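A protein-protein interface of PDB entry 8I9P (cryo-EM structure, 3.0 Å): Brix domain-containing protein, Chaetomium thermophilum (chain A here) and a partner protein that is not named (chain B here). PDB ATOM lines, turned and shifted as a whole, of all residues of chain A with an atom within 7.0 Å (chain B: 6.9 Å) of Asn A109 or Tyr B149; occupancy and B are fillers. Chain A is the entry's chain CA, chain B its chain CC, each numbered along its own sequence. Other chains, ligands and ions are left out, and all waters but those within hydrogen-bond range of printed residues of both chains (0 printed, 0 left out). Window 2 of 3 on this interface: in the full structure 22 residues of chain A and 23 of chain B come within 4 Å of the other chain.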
ATOM      1  N   LYS A 106      -7.628 -19.686  10.331  1.00  0.00           N
ATOM      2  CA  LYS A 106      -7.228 -19.703  11.730  1.00  0.00           C
ATOM      3  C   LYS A 106      -6.641 -21.072  12.040  1.00  0.00           C
ATOM      4  O   LYS A 106      -7.239 -22.101  11.710  1.00  0.00           O
ATOM      5  CB  LYS A 106      -8.422 -19.417  12.638  1.00  0.00           C
ATOM      6  CG  LYS A 106      -9.158 -18.122  12.347  1.00  0.00           C
ATOM      7  CD  LYS A 106      -8.307 -16.912  12.674  1.00  0.00           C
ATOM      8  CE  LYS A 106      -7.938 -16.888  14.148  1.00  0.00           C
ATOM      9  NZ  LYS A 106      -7.415 -15.562  14.568  1.00  0.00           N
ATOM     10  N   VAL A 107      -5.476 -21.087  12.676  1.00  0.00           N
ATOM     11  CA  VAL A 107      -4.640 -22.286  12.716  1.00  0.00           C
ATOM     12  C   VAL A 107      -5.147 -23.377  13.661  1.00  0.00           C
ATOM     13  O   VAL A 107      -5.307 -24.515  13.197  1.00  0.00           O
ATOM     14  CB  VAL A 107      -3.183 -21.909  13.027  1.00  0.00           C
ATOM     15  CG1 VAL A 107      -2.351 -23.150  13.296  1.00  0.00           C
ATOM     16  CG2 VAL A 107      -2.618 -21.118  11.877  1.00  0.00           C
ATOM     17  N   PRO A 108      -5.383 -23.141  14.967  1.00  0.00           N
ATOM     18  CA  PRO A 108      -5.686 -24.296  15.838  1.00  0.00           C
ATOM     19  C   PRO A 108      -7.031 -24.951  15.562  1.00  0.00           C
ATOM     20  O   PRO A 108      -7.080 -26.154  15.269  1.00  0.00           O
ATOM     21  CB  PRO A 108      -5.625 -23.692  17.252  1.00  0.00           C
ATOM     22  CG  PRO A 108      -4.995 -22.349  17.091  1.00  0.00           C
ATOM     23  CD  PRO A 108      -5.446 -21.896  15.754  1.00  0.00           C
ATOM     24  N   ASN A 109      -8.133 -24.192  15.638  1.00  0.00           N
ATOM     25  CA  ASN A 109      -9.447 -24.799  15.447  1.00  0.00           C
ATOM     26  C   ASN A 109     -10.431 -23.917  14.681  1.00  0.00           C
ATOM     27  O   ASN A 109     -11.626 -24.232  14.665  1.00  0.00           O
ATOM     28  CB  ASN A 109     -10.070 -25.165  16.803  1.00  0.00           C
ATOM     29  CG  ASN A 109      -9.389 -26.349  17.457  1.00  0.00           C
ATOM     30  OD1 ASN A 109      -8.921 -26.262  18.592  1.00  0.00           O
ATOM     31  ND2 ASN A 109      -9.333 -27.467  16.743  1.00  0.00           N
ATOM     32  N   GLY A 110      -9.985 -22.835  14.052  1.00  0.00           N
ATOM     33  CA  GLY A 110     -10.902 -21.898  13.447  1.00  0.00           C
ATOM     34  C   GLY A 110     -11.342 -22.309  12.058  1.00  0.00           C
ATOM     35  O   GLY A 110     -10.893 -23.322  11.517  1.00  0.00           O
ATOM     36  N   PRO A 111     -12.194 -21.504  11.362  1.00  0.00           N
ATOM     37  CA  PRO A 111     -12.681 -21.849  10.022  1.00  0.00           C
ATOM     38  C   PRO A 111     -11.649 -21.600   8.912  1.00  0.00           C
ATOM     39  O   PRO A 111     -10.693 -20.880   9.148  1.00  0.00           O
ATOM     40  CB  PRO A 111     -13.879 -20.916   9.775  1.00  0.00           C
ATOM     41  CG  PRO A 111     -14.140 -20.252  11.102  1.00  0.00           C
ATOM     42  CD  PRO A 111     -12.780 -20.205  11.758  1.00  0.00           C
ATOM     43  N   GLU A 247     -15.269 -25.555   8.338  1.00  0.00           N
ATOM     44  CA  GLU A 247     -15.340 -25.383   9.784  1.00  0.00           C
ATOM     45  C   GLU A 247     -14.027 -25.705  10.487  1.00  0.00           C
ATOM     46  O   GLU A 247     -13.665 -25.024  11.451  1.00  0.00           O
ATOM     47  CB  GLU A 247     -16.456 -26.260  10.359  1.00  0.00           C
ATOM     48  CG  GLU A 247     -16.861 -25.913  11.779  1.00  0.00           C
ATOM     49  CD  GLU A 247     -17.259 -27.135  12.580  1.00  0.00           C
ATOM     50  OE1 GLU A 247     -16.447 -28.080  12.667  1.00  0.00           O
ATOM     51  OE2 GLU A 247     -18.385 -27.152  13.120  1.00  0.00           O
ATOM     52  N   GLY A 248     -13.304 -26.721  10.025  1.00  0.00           N
ATOM     53  CA  GLY A 248     -12.059 -27.122  10.643  1.00  0.00           C
ATOM     54  C   GLY A 248     -10.902 -26.224  10.248  1.00  0.00           C
ATOM     55  O   GLY A 248     -11.042 -25.267   9.485  1.00  0.00           O
ATOM     56  N   SER A 249      -9.726 -26.557  10.793  1.00  0.00           N
ATOM     57  CA  SER A 249      -8.525 -25.754  10.567  1.00  0.00           C
ATOM     58  C   SER A 249      -8.119 -25.761   9.099  1.00  0.00           C
ATOM     59  O   SER A 249      -7.925 -24.703   8.490  1.00  0.00           O
ATOM     60  CB  SER A 249      -7.386 -26.271  11.443  1.00  0.00           C
ATOM     61  OG  SER A 249      -7.786 -26.355  12.799  1.00  0.00           O
ATOM     62  N   TYR B 137      -6.544 -33.643  22.114  1.00  0.00           N
ATOM     63  CA  TYR B 137      -7.758 -33.144  21.484  1.00  0.00           C
ATOM     64  C   TYR B 137      -8.927 -33.176  22.465  1.00  0.00           C
ATOM     65  O   TYR B 137      -8.848 -33.746  23.556  1.00  0.00           O
ATOM     66  CB  TYR B 137      -8.073 -33.942  20.216  1.00  0.00           C
ATOM     67  CG  TYR B 137      -8.037 -35.446  20.383  1.00  0.00           C
ATOM     68  CD1 TYR B 137      -9.110 -36.135  20.936  1.00  0.00           C
ATOM     69  CD2 TYR B 137      -6.932 -36.177  19.977  1.00  0.00           C
ATOM     70  CE1 TYR B 137      -9.079 -37.507  21.084  1.00  0.00           C
ATOM     71  CE2 TYR B 137      -6.893 -37.548  20.114  1.00  0.00           C
ATOM     72  CZ  TYR B 137      -7.967 -38.208  20.672  1.00  0.00           C
ATOM     73  OH  TYR B 137      -7.929 -39.575  20.815  1.00  0.00           O
ATOM     74  N   ARG B 138     -10.028 -32.545  22.055  1.00  0.00           N
ATOM     75  CA  ARG B 138     -11.269 -32.532  22.818  1.00  0.00           C
ATOM     76  C   ARG B 138     -12.394 -33.042  21.933  1.00  0.00           C
ATOM     77  O   ARG B 138     -12.455 -32.702  20.748  1.00  0.00           O
ATOM     78  CB  ARG B 138     -11.599 -31.123  23.329  1.00  0.00           C
ATOM     79  CG  ARG B 138     -10.459 -30.435  24.059  1.00  0.00           C
ATOM     80  CD  ARG B 138     -10.961 -29.696  25.287  1.00  0.00           C
ATOM     81  NE  ARG B 138     -11.355 -28.328  24.973  1.00  0.00           N
ATOM     82  CZ  ARG B 138     -12.606 -27.932  24.788  1.00  0.00           C
ATOM     83  NH1 ARG B 138     -13.620 -28.776  24.882  1.00  0.00           N
ATOM     84  NH2 ARG B 138     -12.847 -26.656  24.502  1.00  0.00           N
ATOM     85  N   ILE B 139     -13.280 -33.853  22.507  1.00  0.00           N
ATOM     86  CA  ILE B 139     -14.403 -34.431  21.766  1.00  0.00           C
ATOM     87  C   ILE B 139     -15.522 -33.392  21.752  1.00  0.00           C
ATOM     88  O   ILE B 139     -16.096 -33.066  22.791  1.00  0.00           O
ATOM     89  CB  ILE B 139     -14.874 -35.758  22.370  1.00  0.00           C
ATOM     90  CG1 ILE B 139     -13.789 -36.855  22.353  1.00  0.00           C
ATOM     91  CG2 ILE B 139     -16.122 -36.250  21.649  1.00  0.00           C
ATOM     92  CD1 ILE B 139     -12.737 -36.776  21.246  1.00  0.00           C
ATOM     93  N   GLU B 140     -15.829 -32.866  20.573  1.00  0.00           N
ATOM     94  CA  GLU B 140     -16.886 -31.882  20.383  1.00  0.00           C
ATOM     95  C   GLU B 140     -17.720 -32.270  19.163  1.00  0.00           C
ATOM     96  O   GLU B 140     -17.206 -32.790  18.173  1.00  0.00           O
ATOM     97  CB  GLU B 140     -16.285 -30.473  20.261  1.00  0.00           C
ATOM     98  CG  GLU B 140     -17.122 -29.450  19.502  1.00  0.00           C
ATOM     99  CD  GLU B 140     -16.685 -28.023  19.761  1.00  0.00           C
ATOM    100  OE1 GLU B 140     -15.966 -27.791  20.755  1.00  0.00           O
ATOM    101  OE2 GLU B 140     -17.080 -27.129  18.984  1.00  0.00           O
ATOM    102  N   ASP B 142     -19.680 -31.514  15.868  1.00  0.00           N
ATOM    103  CA  ASP B 142     -19.502 -30.535  14.802  1.00  0.00           C
ATOM    104  C   ASP B 142     -20.863 -30.008  14.347  1.00  0.00           C
ATOM    105  O   ASP B 142     -21.907 -30.329  14.923  1.00  0.00           O
ATOM    106  CB  ASP B 142     -18.711 -31.150  13.652  1.00  0.00           C
ATOM    107  CG  ASP B 142     -19.575 -31.996  12.742  1.00  0.00           C
ATOM    108  OD1 ASP B 142     -20.227 -32.925  13.252  1.00  0.00           O
ATOM    109  OD2 ASP B 142     -19.604 -31.732  11.523  1.00  0.00           O
ATOM    110  N   ILE B 147     -17.983 -35.931  14.294  1.00  0.00           N
ATOM    111  CA  ILE B 147     -16.950 -35.790  15.313  1.00  0.00           C
ATOM    112  C   ILE B 147     -16.066 -34.609  14.945  1.00  0.00           C
ATOM    113  O   ILE B 147     -15.569 -34.527  13.816  1.00  0.00           O
ATOM    114  CB  ILE B 147     -16.107 -37.074  15.453  1.00  0.00           C
ATOM    115  CG1 ILE B 147     -16.966 -38.228  15.970  1.00  0.00           C
ATOM    116  CG2 ILE B 147     -14.924 -36.849  16.382  1.00  0.00           C
ATOM    117  CD1 ILE B 147     -16.252 -39.558  15.983  1.00  0.00           C
ATOM    118  N   ARG B 148     -15.874 -33.695  15.892  1.00  0.00           N
ATOM    119  CA  ARG B 148     -14.954 -32.579  15.738  1.00  0.00           C
ATOM    120  C   ARG B 148     -13.916 -32.611  16.851  1.00  0.00           C
ATOM    121  O   ARG B 148     -14.226 -32.928  18.003  1.00  0.00           O
ATOM    122  CB  ARG B 148     -15.685 -31.236  15.757  1.00  0.00           C
ATOM    123  CG  ARG B 148     -14.834 -30.097  15.257  1.00  0.00           C
ATOM    124  CD  ARG B 148     -14.999 -28.868  16.114  1.00  0.00           C
ATOM    125  NE  ARG B 148     -14.553 -27.683  15.397  1.00  0.00           N
ATOM    126  CZ  ARG B 148     -13.373 -27.107  15.577  1.00  0.00           C
ATOM    127  NH1 ARG B 148     -12.511 -27.562  16.470  1.00  0.00           N
ATOM    128  NH2 ARG B 148     -13.046 -26.053  14.836  1.00  0.00           N
ATOM    129  N   TYR B 149     -12.678 -32.279  16.494  1.00  0.00           N
ATOM    130  CA  TYR B 149     -11.551 -32.312  17.416  1.00  0.00           C
ATOM    131  C   TYR B 149     -11.125 -30.884  17.722  1.00  0.00           C
ATOM    132  O   TYR B 149     -10.911 -30.087  16.803  1.00  0.00           O
ATOM    133  CB  TYR B 149     -10.391 -33.106  16.820  1.00  0.00           C
ATOM    134  CG  TYR B 149     -10.621 -34.597  16.829  1.00  0.00           C
ATOM    135  CD1 TYR B 149     -10.858 -35.275  18.015  1.00  0.00           C
ATOM    136  CD2 TYR B 149     -10.619 -35.325  15.646  1.00  0.00           C
ATOM    137  CE1 TYR B 149     -11.075 -36.640  18.025  1.00  0.00           C
ATOM    138  CE2 TYR B 149     -10.835 -36.688  15.646  1.00  0.00           C
ATOM    139  CZ  TYR B 149     -11.062 -37.340  16.838  1.00  0.00           C
ATOM    140  OH  TYR B 149     -11.278 -38.698  16.844  1.00  0.00           O
ATOM    141  N   VAL B 150     -11.003 -30.564  19.006  1.00  0.00           N
ATOM    142  CA  VAL B 150     -10.569 -29.248  19.456  1.00  0.00           C
ATOM    143  C   VAL B 150      -9.197 -29.397  20.097  1.00  0.00           C
ATOM    144  O   VAL B 150      -9.039 -30.128  21.082  1.00  0.00           O
ATOM    145  CB  VAL B 150     -11.574 -28.629  20.437  1.00  0.00           C
ATOM    146  CG1 VAL B 150     -11.055 -27.299  20.957  1.00  0.00           C
ATOM    147  CG2 VAL B 150     -12.917 -28.450  19.762  1.00  0.00           C
ATOM    148  N   TYR B 151      -8.210 -28.702  19.547  1.00  0.00           N
ATOM    149  CA  TYR B 151      -6.833 -28.790  20.005  1.00  0.00           C
ATOM    150  C   TYR B 151      -6.499 -27.595  20.886  1.00  0.00           C
ATOM    151  O   TYR B 151      -7.300 -26.670  21.047  1.00  0.00           O
ATOM    152  CB  TYR B 151      -5.869 -28.858  18.817  1.00  0.00           C
ATOM    153  CG  TYR B 151      -6.161 -30.001  17.872  1.00  0.00           C
ATOM    154  CD1 TYR B 151      -5.695 -31.282  18.136  1.00  0.00           C
ATOM    155  CD2 TYR B 151      -6.910 -29.799  16.722  1.00  0.00           C
ATOM    156  CE1 TYR B 151      -5.965 -32.329  17.275  1.00  0.00           C
ATOM    157  CE2 TYR B 151      -7.187 -30.839  15.860  1.00  0.00           C
ATOM    158  CZ  TYR B 151      -6.712 -32.100  16.140  1.00  0.00           C
ATOM    159  OH  TYR B 151      -6.986 -33.136  15.277  1.00  0.00           O
ATOM    160  N   ASP B 152      -5.303 -27.635  21.467  1.00  0.00           N
ATOM    161  CA  ASP B 152      -4.830 -26.530  22.291  1.00  0.00           C
ATOM    162  C   ASP B 152      -4.576 -25.301  21.431  1.00  0.00           C
ATOM    163  O   ASP B 152      -3.946 -25.386  20.374  1.00  0.00           O
ATOM    164  CB  ASP B 152      -3.556 -26.936  23.030  1.00  0.00           C
ATOM    165  CG  ASP B 152      -3.700 -28.261  23.751  1.00  0.00           C
ATOM    166  OD1 ASP B 152      -4.479 -29.114  23.276  1.00  0.00           O
ATOM    167  OD2 ASP B 152      -3.035 -28.449  24.792  1.00  0.00           O
ATOM    168  N   GLU B 153      -5.079 -24.158  21.888  1.00  0.00           N
ATOM    169  CA  GLU B 153      -4.955 -22.926  21.128  1.00  0.00           C
ATOM    170  C   GLU B 153      -3.509 -22.436  21.133  1.00  0.00           C
ATOM    171  O   GLU B 153      -2.742 -22.667  22.071  1.00  0.00           O
ATOM    172  CB  GLU B 153      -5.883 -21.853  21.693  1.00  0.00           C
ATOM    173  CG  GLU B 153      -6.498 -20.951  20.636  1.00  0.00           C
ATOM    174  CD  GLU B 153      -7.832 -21.468  20.134  1.00  0.00           C
ATOM    175  OE1 GLU B 153      -8.813 -21.430  20.906  1.00  0.00           O
ATOM    176  OE2 GLU B 153      -7.900 -21.914  18.971  1.00  0.00           O
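The guanidinium group of Arg B148 lies within salt-bridge range of the side-chain carboxylate of Glu A247 (3.3 Å).
ND2 of Asn A109 sits at hydrogen-bond distance from O of Tyr B149 (3.1 Å).
The guanidinium group (NH1) of Arg B148 lies close to the side-chain amide nitrogen (ND2) of Asn A109, 3.2 Å away.
The side-chain amide oxygen of Asn A109 sits at hydrogen-bond distance from the backbone NH of Tyr B151.
Of the 12 printed residues of chain B, 7 touch a printed residue of chain A.
Hydrophobic or aromatic side chains of chain B within 4 Å of the printed part of chain A: Val B150 and Tyr B151.
Hydrophobic or aromatic side chains of chain A that line the printed part of chain B: Pro A108.
Along chain A the printed residues that touch a printed residue of chain B span positions 108 to 247.
Among the printed residues, Asp or Glu carboxylates within 4 Å of a Lys or Arg side-chain nitrogen of the other chain: Glu A247 with Arg B148 (3.3 Å).
OG of Ser A249 lies within hydrogen-bond range of O of Pro A108, 2.6 Å away.
The backbone carbonyl oxygen (O) of Glu B140 is in hydrogen-bond range of the backbone NH (N) of Arg B148 (2.8 Å).
The backbone NH (N) of Arg B138 is in hydrogen-bond range of the backbone carbonyl oxygen (O) of Val B150, at 2.8 Å.
Lys A106 touches none of the printed residues of chain B.
Printed residues of chain B within 4 Å of Pro A108: Tyr B151, Asp B152 and Glu B153.
Asn A109 touches just these residues of chain B: Arg B148, Tyr B149, Val B150 and Tyr B151.
Ile B139 touches none of the printed residues of chain A.
Of the printed residues of chain A, Arg B148 touches Asn A109 and Glu A247.
Tyr B149 touches one residue of chain A.
Printed residues of chain A within 4 Å of Tyr B151: Pro A108 (3.9 Å) and Asn A109 (2.7 Å).
The nearest residue of chain A that does not touch Tyr B149 is Pro A108 (5.7 Å).
The nearest printed residue of chain A that does not touch Val B150 is Pro A108 (6.2 Å).
Among the printed residues, pairs that only touch across the chains: Asn A109 with Val B150 (3.4 Å), Pro A108 with Glu B153 (3.4 Å), Pro A108 with Tyr B151 (3.9 Å), Pro A108 with Asp B152 (3.9 Å) and Glu A247 with Asp B142 (3.9 Å).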
